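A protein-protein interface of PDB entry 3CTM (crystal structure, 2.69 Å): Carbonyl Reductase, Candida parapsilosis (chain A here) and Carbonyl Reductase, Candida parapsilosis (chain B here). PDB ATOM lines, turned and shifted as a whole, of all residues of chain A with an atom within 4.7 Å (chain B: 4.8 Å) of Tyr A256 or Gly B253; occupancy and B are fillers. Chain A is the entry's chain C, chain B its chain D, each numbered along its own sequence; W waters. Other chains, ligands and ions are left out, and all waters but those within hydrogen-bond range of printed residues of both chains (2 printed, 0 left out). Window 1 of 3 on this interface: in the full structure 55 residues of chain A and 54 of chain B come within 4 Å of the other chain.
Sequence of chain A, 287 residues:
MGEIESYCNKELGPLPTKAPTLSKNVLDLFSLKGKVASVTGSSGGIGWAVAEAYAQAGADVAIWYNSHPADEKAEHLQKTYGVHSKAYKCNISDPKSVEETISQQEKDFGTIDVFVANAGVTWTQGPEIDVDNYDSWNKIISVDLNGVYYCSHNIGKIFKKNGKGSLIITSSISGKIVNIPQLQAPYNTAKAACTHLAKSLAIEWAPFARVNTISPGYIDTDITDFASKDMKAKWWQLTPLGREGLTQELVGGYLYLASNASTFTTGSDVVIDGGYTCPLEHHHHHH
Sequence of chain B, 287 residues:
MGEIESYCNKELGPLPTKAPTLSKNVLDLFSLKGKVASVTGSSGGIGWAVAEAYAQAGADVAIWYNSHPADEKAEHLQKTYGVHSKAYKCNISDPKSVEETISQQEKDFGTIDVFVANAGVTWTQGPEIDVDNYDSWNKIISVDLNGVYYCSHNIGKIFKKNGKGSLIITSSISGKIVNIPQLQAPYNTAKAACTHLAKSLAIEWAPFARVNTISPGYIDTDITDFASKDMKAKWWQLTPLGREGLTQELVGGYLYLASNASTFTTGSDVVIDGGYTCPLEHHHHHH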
ATOM      1  N   PHE A  30      -8.464  -8.057   7.209  1.00  0.00           N
ATOM      2  CA  PHE A  30      -7.623  -7.468   6.182  1.00  0.00           C
ATOM      3  C   PHE A  30      -6.704  -6.394   6.726  1.00  0.00           C
ATOM      4  O   PHE A  30      -5.990  -5.756   5.952  1.00  0.00           O
ATOM      5  CB  PHE A  30      -8.480  -6.910   5.042  1.00  0.00           C
ATOM      6  CG  PHE A  30      -9.167  -7.984   4.238  1.00  0.00           C
ATOM      7  CD1 PHE A  30     -10.395  -8.485   4.630  1.00  0.00           C
ATOM      8  CD2 PHE A  30      -8.566  -8.518   3.120  1.00  0.00           C
ATOM      9  CE1 PHE A  30     -11.015  -9.483   3.915  1.00  0.00           C
ATOM     10  CE2 PHE A  30      -9.187  -9.526   2.399  1.00  0.00           C
ATOM     11  CZ  PHE A  30     -10.413  -9.999   2.788  1.00  0.00           C
ATOM     12  N   GLY A 252      -6.204  -5.798  -4.230  1.00  0.00           N
ATOM     13  CA  GLY A 252      -7.016  -6.491  -3.247  1.00  0.00           C
ATOM     14  C   GLY A 252      -6.518  -7.900  -2.991  1.00  0.00           C
ATOM     15  O   GLY A 252      -6.536  -8.379  -1.852  1.00  0.00           O
ATOM     16  N   GLY A 253      -6.077  -8.589  -4.046  1.00  0.00           N
ATOM     17  CA  GLY A 253      -5.574  -9.935  -3.870  1.00  0.00           C
ATOM     18  C   GLY A 253      -4.266  -9.958  -3.105  1.00  0.00           C
ATOM     19  O   GLY A 253      -4.007 -10.876  -2.309  1.00  0.00           O
ATOM     20  N   TYR A 254      -3.412  -8.958  -3.339  1.00  0.00           N
ATOM     21  CA  TYR A 254      -2.174  -8.903  -2.579  1.00  0.00           C
ATOM     22  C   TYR A 254      -2.458  -8.677  -1.106  1.00  0.00           C
ATOM     23  O   TYR A 254      -1.652  -9.063  -0.251  1.00  0.00           O
ATOM     24  CB  TYR A 254      -1.241  -7.820  -3.132  1.00  0.00           C
ATOM     25  CG  TYR A 254      -0.428  -8.287  -4.334  1.00  0.00           C
ATOM     26  CD1 TYR A 254      -0.917  -8.141  -5.637  1.00  0.00           C
ATOM     27  CD2 TYR A 254       0.813  -8.900  -4.163  1.00  0.00           C
ATOM     28  CE1 TYR A 254      -0.189  -8.583  -6.740  1.00  0.00           C
ATOM     29  CE2 TYR A 254       1.546  -9.344  -5.257  1.00  0.00           C
ATOM     30  CZ  TYR A 254       1.043  -9.183  -6.552  1.00  0.00           C
ATOM     31  OH  TYR A 254       1.774  -9.623  -7.648  1.00  0.00           O
ATOM     32  N   LEU A 255      -3.605  -8.076  -0.787  1.00  0.00           N
ATOM     33  CA  LEU A 255      -3.970  -7.887   0.610  1.00  0.00           C
ATOM     34  C   LEU A 255      -4.663  -9.124   1.176  1.00  0.00           C
ATOM     35  O   LEU A 255      -4.425  -9.487   2.332  1.00  0.00           O
ATOM     36  CB  LEU A 255      -4.856  -6.652   0.761  1.00  0.00           C
ATOM     37  CG  LEU A 255      -5.265  -6.344   2.188  1.00  0.00           C
ATOM     38  CD1 LEU A 255      -4.074  -5.964   3.029  1.00  0.00           C
ATOM     39  CD2 LEU A 255      -6.250  -5.236   2.143  1.00  0.00           C
ATOM     40  N   TYR A 256      -5.506  -9.793   0.380  1.00  0.00           N
ATOM     41  CA  TYR A 256      -6.052 -11.079   0.811  1.00  0.00           C
ATOM     42  C   TYR A 256      -4.961 -12.053   1.258  1.00  0.00           C
ATOM     43  O   TYR A 256      -5.114 -12.733   2.274  1.00  0.00           O
ATOM     44  CB  TYR A 256      -6.868 -11.725  -0.298  1.00  0.00           C
ATOM     45  CG  TYR A 256      -7.225 -13.169  -0.002  1.00  0.00           C
ATOM     46  CD1 TYR A 256      -8.091 -13.492   1.034  1.00  0.00           C
ATOM     47  CD2 TYR A 256      -6.710 -14.210  -0.766  1.00  0.00           C
ATOM     48  CE1 TYR A 256      -8.448 -14.813   1.299  1.00  0.00           C
ATOM     49  CE2 TYR A 256      -7.049 -15.540  -0.509  1.00  0.00           C
ATOM     50  CZ  TYR A 256      -7.928 -15.843   0.525  1.00  0.00           C
ATOM     51  OH  TYR A 256      -8.266 -17.174   0.791  1.00  0.00           O
ATOM     52  N   LEU A 257      -3.854 -12.136   0.509  1.00  0.00           N
ATOM     53  CA  LEU A 257      -2.826 -13.137   0.792  1.00  0.00           C
ATOM     54  C   LEU A 257      -1.913 -12.737   1.945  1.00  0.00           C
ATOM     55  O   LEU A 257      -1.363 -13.612   2.621  1.00  0.00           O
ATOM     56  CB  LEU A 257      -1.984 -13.397  -0.457  1.00  0.00           C
ATOM     57  CG  LEU A 257      -2.705 -14.214  -1.531  1.00  0.00           C
ATOM     58  CD1 LEU A 257      -1.865 -14.350  -2.765  1.00  0.00           C
ATOM     59  CD2 LEU A 257      -3.096 -15.565  -0.993  1.00  0.00           C
ATOM     60  N   ALA A 258      -1.742 -11.444   2.190  1.00  0.00           N
ATOM     61  CA  ALA A 258      -0.805 -10.974   3.202  1.00  0.00           C
ATOM     62  C   ALA A 258      -1.406 -10.909   4.592  1.00  0.00           C
ATOM     63  O   ALA A 258      -0.667 -10.987   5.573  1.00  0.00           O
ATOM     64  CB  ALA A 258      -0.278  -9.583   2.830  1.00  0.00           C
ATOM     65  N   SER A 259      -2.714 -10.771   4.691  1.00  0.00           N
ATOM     66  CA  SER A 259      -3.410 -10.433   5.916  1.00  0.00           C
ATOM     67  C   SER A 259      -3.987 -11.692   6.551  1.00  0.00           C
ATOM     68  O   SER A 259      -3.930 -12.780   5.981  1.00  0.00           O
ATOM     69  CB  SER A 259      -4.522  -9.427   5.609  1.00  0.00           C
ATOM     70  OG  SER A 259      -5.607 -10.092   4.977  1.00  0.00           O
ATOM     71  N   ALA A 261      -6.821 -12.538   6.487  1.00  0.00           N
ATOM     72  CA  ALA A 261      -7.920 -13.063   5.692  1.00  0.00           C
ATOM     73  C   ALA A 261      -7.623 -14.453   5.128  1.00  0.00           C
ATOM     74  O   ALA A 261      -8.557 -15.173   4.744  1.00  0.00           O
ATOM     75  CB  ALA A 261      -8.227 -12.093   4.557  1.00  0.00           C
ATOM     76  N   SER A 262      -6.349 -14.848   5.058  1.00  0.00           N
ATOM     77  CA  SER A 262      -5.967 -16.053   4.333  1.00  0.00           C
ATOM     78  C   SER A 262      -5.156 -17.005   5.197  1.00  0.00           C
ATOM     79  O   SER A 262      -4.293 -17.717   4.676  1.00  0.00           O
ATOM     80  CB  SER A 262      -5.174 -15.703   3.082  1.00  0.00           C
ATOM     81  OG  SER A 262      -4.045 -14.903   3.415  1.00  0.00           O
ATOM     82  N   THR A 265      -4.743 -20.303   3.758  1.00  0.00           N
ATOM     83  CA  THR A 265      -4.437 -20.339   2.334  1.00  0.00           C
ATOM     84  C   THR A 265      -2.928 -20.399   2.116  1.00  0.00           C
ATOM     85  O   THR A 265      -2.219 -19.410   2.338  1.00  0.00           O
ATOM     86  CB  THR A 265      -5.033 -19.129   1.626  1.00  0.00           C
ATOM     87  OG1 THR A 265      -6.434 -19.054   1.931  1.00  0.00           O
ATOM     88  CG2 THR A 265      -4.804 -19.242   0.110  1.00  0.00           C
ATOM     89  N   ILE B 214     -15.055 -20.923  -5.114  1.00  0.00           N
ATOM     90  CA  ILE B 214     -14.282 -21.093  -3.899  1.00  0.00           C
ATOM     91  C   ILE B 214     -14.172 -22.590  -3.668  1.00  0.00           C
ATOM     92  O   ILE B 214     -15.176 -23.312  -3.782  1.00  0.00           O
ATOM     93  CB  ILE B 214     -14.943 -20.389  -2.698  1.00  0.00           C
ATOM     94  CG1 ILE B 214     -14.797 -18.882  -2.802  1.00  0.00           C
ATOM     95  CG2 ILE B 214     -14.334 -20.875  -1.385  1.00  0.00           C
ATOM     96  CD1 ILE B 214     -13.508 -18.363  -2.188  1.00  0.00           C
ATOM     97  N   LEU B 250     -12.426 -19.142   5.542  1.00  0.00           N
ATOM     98  CA  LEU B 250     -12.994 -19.010   4.208  1.00  0.00           C
ATOM     99  C   LEU B 250     -13.575 -17.634   3.962  1.00  0.00           C
ATOM    100  O   LEU B 250     -13.591 -17.147   2.825  1.00  0.00           O
ATOM    101  CB  LEU B 250     -14.097 -20.042   4.004  1.00  0.00           C
ATOM    102  CG  LEU B 250     -13.664 -21.462   4.298  1.00  0.00           C
ATOM    103  CD1 LEU B 250     -14.893 -22.333   4.439  1.00  0.00           C
ATOM    104  CD2 LEU B 250     -12.773 -21.922   3.153  1.00  0.00           C
ATOM    105  N   VAL B 251     -14.007 -16.993   5.031  1.00  0.00           N
ATOM    106  CA  VAL B 251     -14.824 -15.787   4.956  1.00  0.00           C
ATOM    107  C   VAL B 251     -14.120 -14.672   4.169  1.00  0.00           C
ATOM    108  O   VAL B 251     -14.751 -13.950   3.385  1.00  0.00           O
ATOM    109  CB  VAL B 251     -15.194 -15.398   6.403  1.00  0.00           C
ATOM    110  CG1 VAL B 251     -14.786 -13.994   6.762  1.00  0.00           C
ATOM    111  CG2 VAL B 251     -16.659 -15.694   6.660  1.00  0.00           C
ATOM    112  N   GLY B 252     -12.804 -14.539   4.330  1.00  0.00           N
ATOM    113  CA  GLY B 252     -12.101 -13.478   3.631  1.00  0.00           C
ATOM    114  C   GLY B 252     -12.039 -13.712   2.134  1.00  0.00           C
ATOM    115  O   GLY B 252     -12.127 -12.765   1.338  1.00  0.00           O
ATOM    116  N   GLY B 253     -11.880 -14.976   1.728  1.00  0.00           N
ATOM    117  CA  GLY B 253     -11.928 -15.298   0.313  1.00  0.00           C
ATOM    118  C   GLY B 253     -13.269 -14.948  -0.298  1.00  0.00           C
ATOM    119  O   GLY B 253     -13.335 -14.427  -1.417  1.00  0.00           O
ATOM    120  N   TYR B 254     -14.362 -15.210   0.437  1.00  0.00           N
ATOM    121  CA  TYR B 254     -15.669 -14.834  -0.089  1.00  0.00           C
ATOM    122  C   TYR B 254     -15.827 -13.323  -0.156  1.00  0.00           C
ATOM    123  O   TYR B 254     -16.501 -12.818  -1.063  1.00  0.00           O
ATOM    124  CB  TYR B 254     -16.795 -15.446   0.738  1.00  0.00           C
ATOM    125  CG  TYR B 254     -16.992 -16.927   0.506  1.00  0.00           C
ATOM    126  CD1 TYR B 254     -16.184 -17.857   1.148  1.00  0.00           C
ATOM    127  CD2 TYR B 254     -17.981 -17.392  -0.345  1.00  0.00           C
ATOM    128  CE1 TYR B 254     -16.356 -19.193   0.958  1.00  0.00           C
ATOM    129  CE2 TYR B 254     -18.158 -18.738  -0.549  1.00  0.00           C
ATOM    130  CZ  TYR B 254     -17.342 -19.635   0.102  1.00  0.00           C
ATOM    131  OH  TYR B 254     -17.499 -20.982  -0.089  1.00  0.00           O
ATOM    132  N   LEU B 255     -15.218 -12.576   0.773  1.00  0.00           N
ATOM    133  CA  LEU B 255     -15.359 -11.127   0.681  1.00  0.00           C
ATOM    134  C   LEU B 255     -14.611 -10.596  -0.536  1.00  0.00           C
ATOM    135  O   LEU B 255     -15.104  -9.701  -1.245  1.00  0.00           O
ATOM    136  CB  LEU B 255     -14.866 -10.445   1.958  1.00  0.00           C
ATOM    137  CG  LEU B 255     -15.704  -9.274   2.485  1.00  0.00           C
ATOM    138  CD1 LEU B 255     -14.823  -8.201   3.098  1.00  0.00           C
ATOM    139  CD2 LEU B 255     -16.622  -8.672   1.409  1.00  0.00           C
ATOM    140  N   TYR B 256     -13.424 -11.157  -0.795  1.00  0.00           N
ATOM    141  CA  TYR B 256     -12.618 -10.728  -1.928  1.00  0.00           C
ATOM    142  C   TYR B 256     -13.404 -10.877  -3.221  1.00  0.00           C
ATOM    143  O   TYR B 256     -13.553  -9.915  -3.990  1.00  0.00           O
ATOM    144  CB  TYR B 256     -11.315 -11.538  -1.962  1.00  0.00           C
ATOM    145  CG  TYR B 256     -10.497 -11.365  -3.220  1.00  0.00           C
ATOM    146  CD1 TYR B 256      -9.690 -10.254  -3.395  1.00  0.00           C
ATOM    147  CD2 TYR B 256     -10.528 -12.323  -4.237  1.00  0.00           C
ATOM    148  CE1 TYR B 256      -8.943 -10.098  -4.531  1.00  0.00           C
ATOM    149  CE2 TYR B 256      -9.788 -12.167  -5.381  1.00  0.00           C
ATOM    150  CZ  TYR B 256      -9.001 -11.050  -5.525  1.00  0.00           C
ATOM    151  OH  TYR B 256      -8.257 -10.876  -6.672  1.00  0.00           O
ATOM    152  N   LEU B 257     -13.966 -12.070  -3.442  1.00  0.00           N
ATOM    153  CA  LEU B 257     -14.644 -12.353  -4.699  1.00  0.00           C
ATOM    154  C   LEU B 257     -15.915 -11.538  -4.836  1.00  0.00           C
ATOM    155  O   LEU B 257     -16.205 -11.018  -5.922  1.00  0.00           O
ATOM    156  CB  LEU B 257     -14.954 -13.841  -4.814  1.00  0.00           C
ATOM    157  CG  LEU B 257     -13.745 -14.756  -5.000  1.00  0.00           C
ATOM    158  CD1 LEU B 257     -14.193 -16.217  -5.093  1.00  0.00           C
ATOM    159  CD2 LEU B 257     -12.907 -14.318  -6.214  1.00  0.00           C
ATOM    160  N   VAL B 270     -10.427 -20.008  -6.297  1.00  0.00           N
ATOM    161  CA  VAL B 270      -9.638 -19.663  -5.122  1.00  0.00           C
ATOM    162  C   VAL B 270      -9.642 -20.870  -4.189  1.00  0.00           C
ATOM    163  O   VAL B 270     -10.686 -21.250  -3.654  1.00  0.00           O
ATOM    164  CB  VAL B 270     -10.172 -18.409  -4.424  1.00  0.00           C
ATOM    165  CG1 VAL B 270      -9.397 -18.164  -3.127  1.00  0.00           C
ATOM    166  CG2 VAL B 270     -10.043 -17.208  -5.338  1.00  0.00           C
ATOM    167  N   ILE B 272      -8.605 -22.892  -0.825  1.00  0.00           N
ATOM    168  CA  ILE B 272      -8.358 -22.584   0.586  1.00  0.00           C
ATOM    169  C   ILE B 272      -8.311 -23.900   1.354  1.00  0.00           C
ATOM    170  O   ILE B 272      -9.284 -24.308   1.998  1.00  0.00           O
ATOM    171  CB  ILE B 272      -9.423 -21.628   1.175  1.00  0.00           C
ATOM    172  CG1 ILE B 272      -9.548 -20.339   0.354  1.00  0.00           C
ATOM    173  CG2 ILE B 272      -9.071 -21.253   2.614  1.00  0.00           C
ATOM    174  CD1 ILE B 272     -10.818 -19.553   0.630  1.00  0.00           C
HETATM  175  O   HOH W   1      -9.908 -16.843   3.104  1.00  0.00           O
HETATM  176  O   HOH W   2      -7.249  -8.201  -6.818  1.00  0.00           O
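Of chain B, only Gly B252 (3.8 Å), Gly B253 (3.5 Å) and Ile B272 (3.4 Å) come within 4 Å of Tyr A256.
Gly B253 touches one residue of chain A.
Printed residues of chain A within 4 Å of Ile B272: Tyr A256 (3.4 Å) and Thr A265 (3.5 Å).
Of the printed residues of chain B, Gly A253 touches Tyr B256.
Val B251 touches none of the printed residues of chain A.
The nearest residue of chain A that does not touch Gly B253 is Ala A261 (4.5 Å).
The nearest printed residue of chain B that does not touch Gly A252 is Gly B252 (7.8 Å).
Among the printed residues, merely in contact across the chains: Gly A253 with Tyr B256 (3.3 Å), Tyr A256 with Ile B272 (3.4 Å), Tyr A256 with Gly B253 (3.5 Å), Thr A265 with Ile B272 (3.5 Å), Phe A30 with Gly B252 (3.6 Å), Gly A252 with Tyr B256 (3.6 Å) and Tyr A256 with Gly B252 (3.8 Å).
Of the 12 printed residues of chain A, 5 touch a printed residue of chain B.
Hydrophobic or aromatic side chains of chain B that line the printed part of chain A: Tyr B256 and Ile B272.
Among the printed residues, no Asp or Glu carboxylate lies within 4 Å of a Lys or Arg side-chain nitrogen of the other chain.
OG of Ser A262 lies within hydrogen-bond range of O of Tyr A256 (2.7 Å).
The side-chain hydroxyl of Tyr A256 sits at hydrogen-bond distance from the side-chain hydroxyl of Thr A265, at 2.9 Å.
Water W1 lies within hydrogen-bond range of the backbone carbonyl oxygen of Ala A261 (2.7 Å), the side-chain hydroxyl of Tyr A256 (2.9 Å) and the backbone NH of Gly B253 (3.0 Å).
Water W2 lies within hydrogen-bond range of OH of Tyr B256 (2.9 Å) and N of Gly A253 (3.0 Å).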
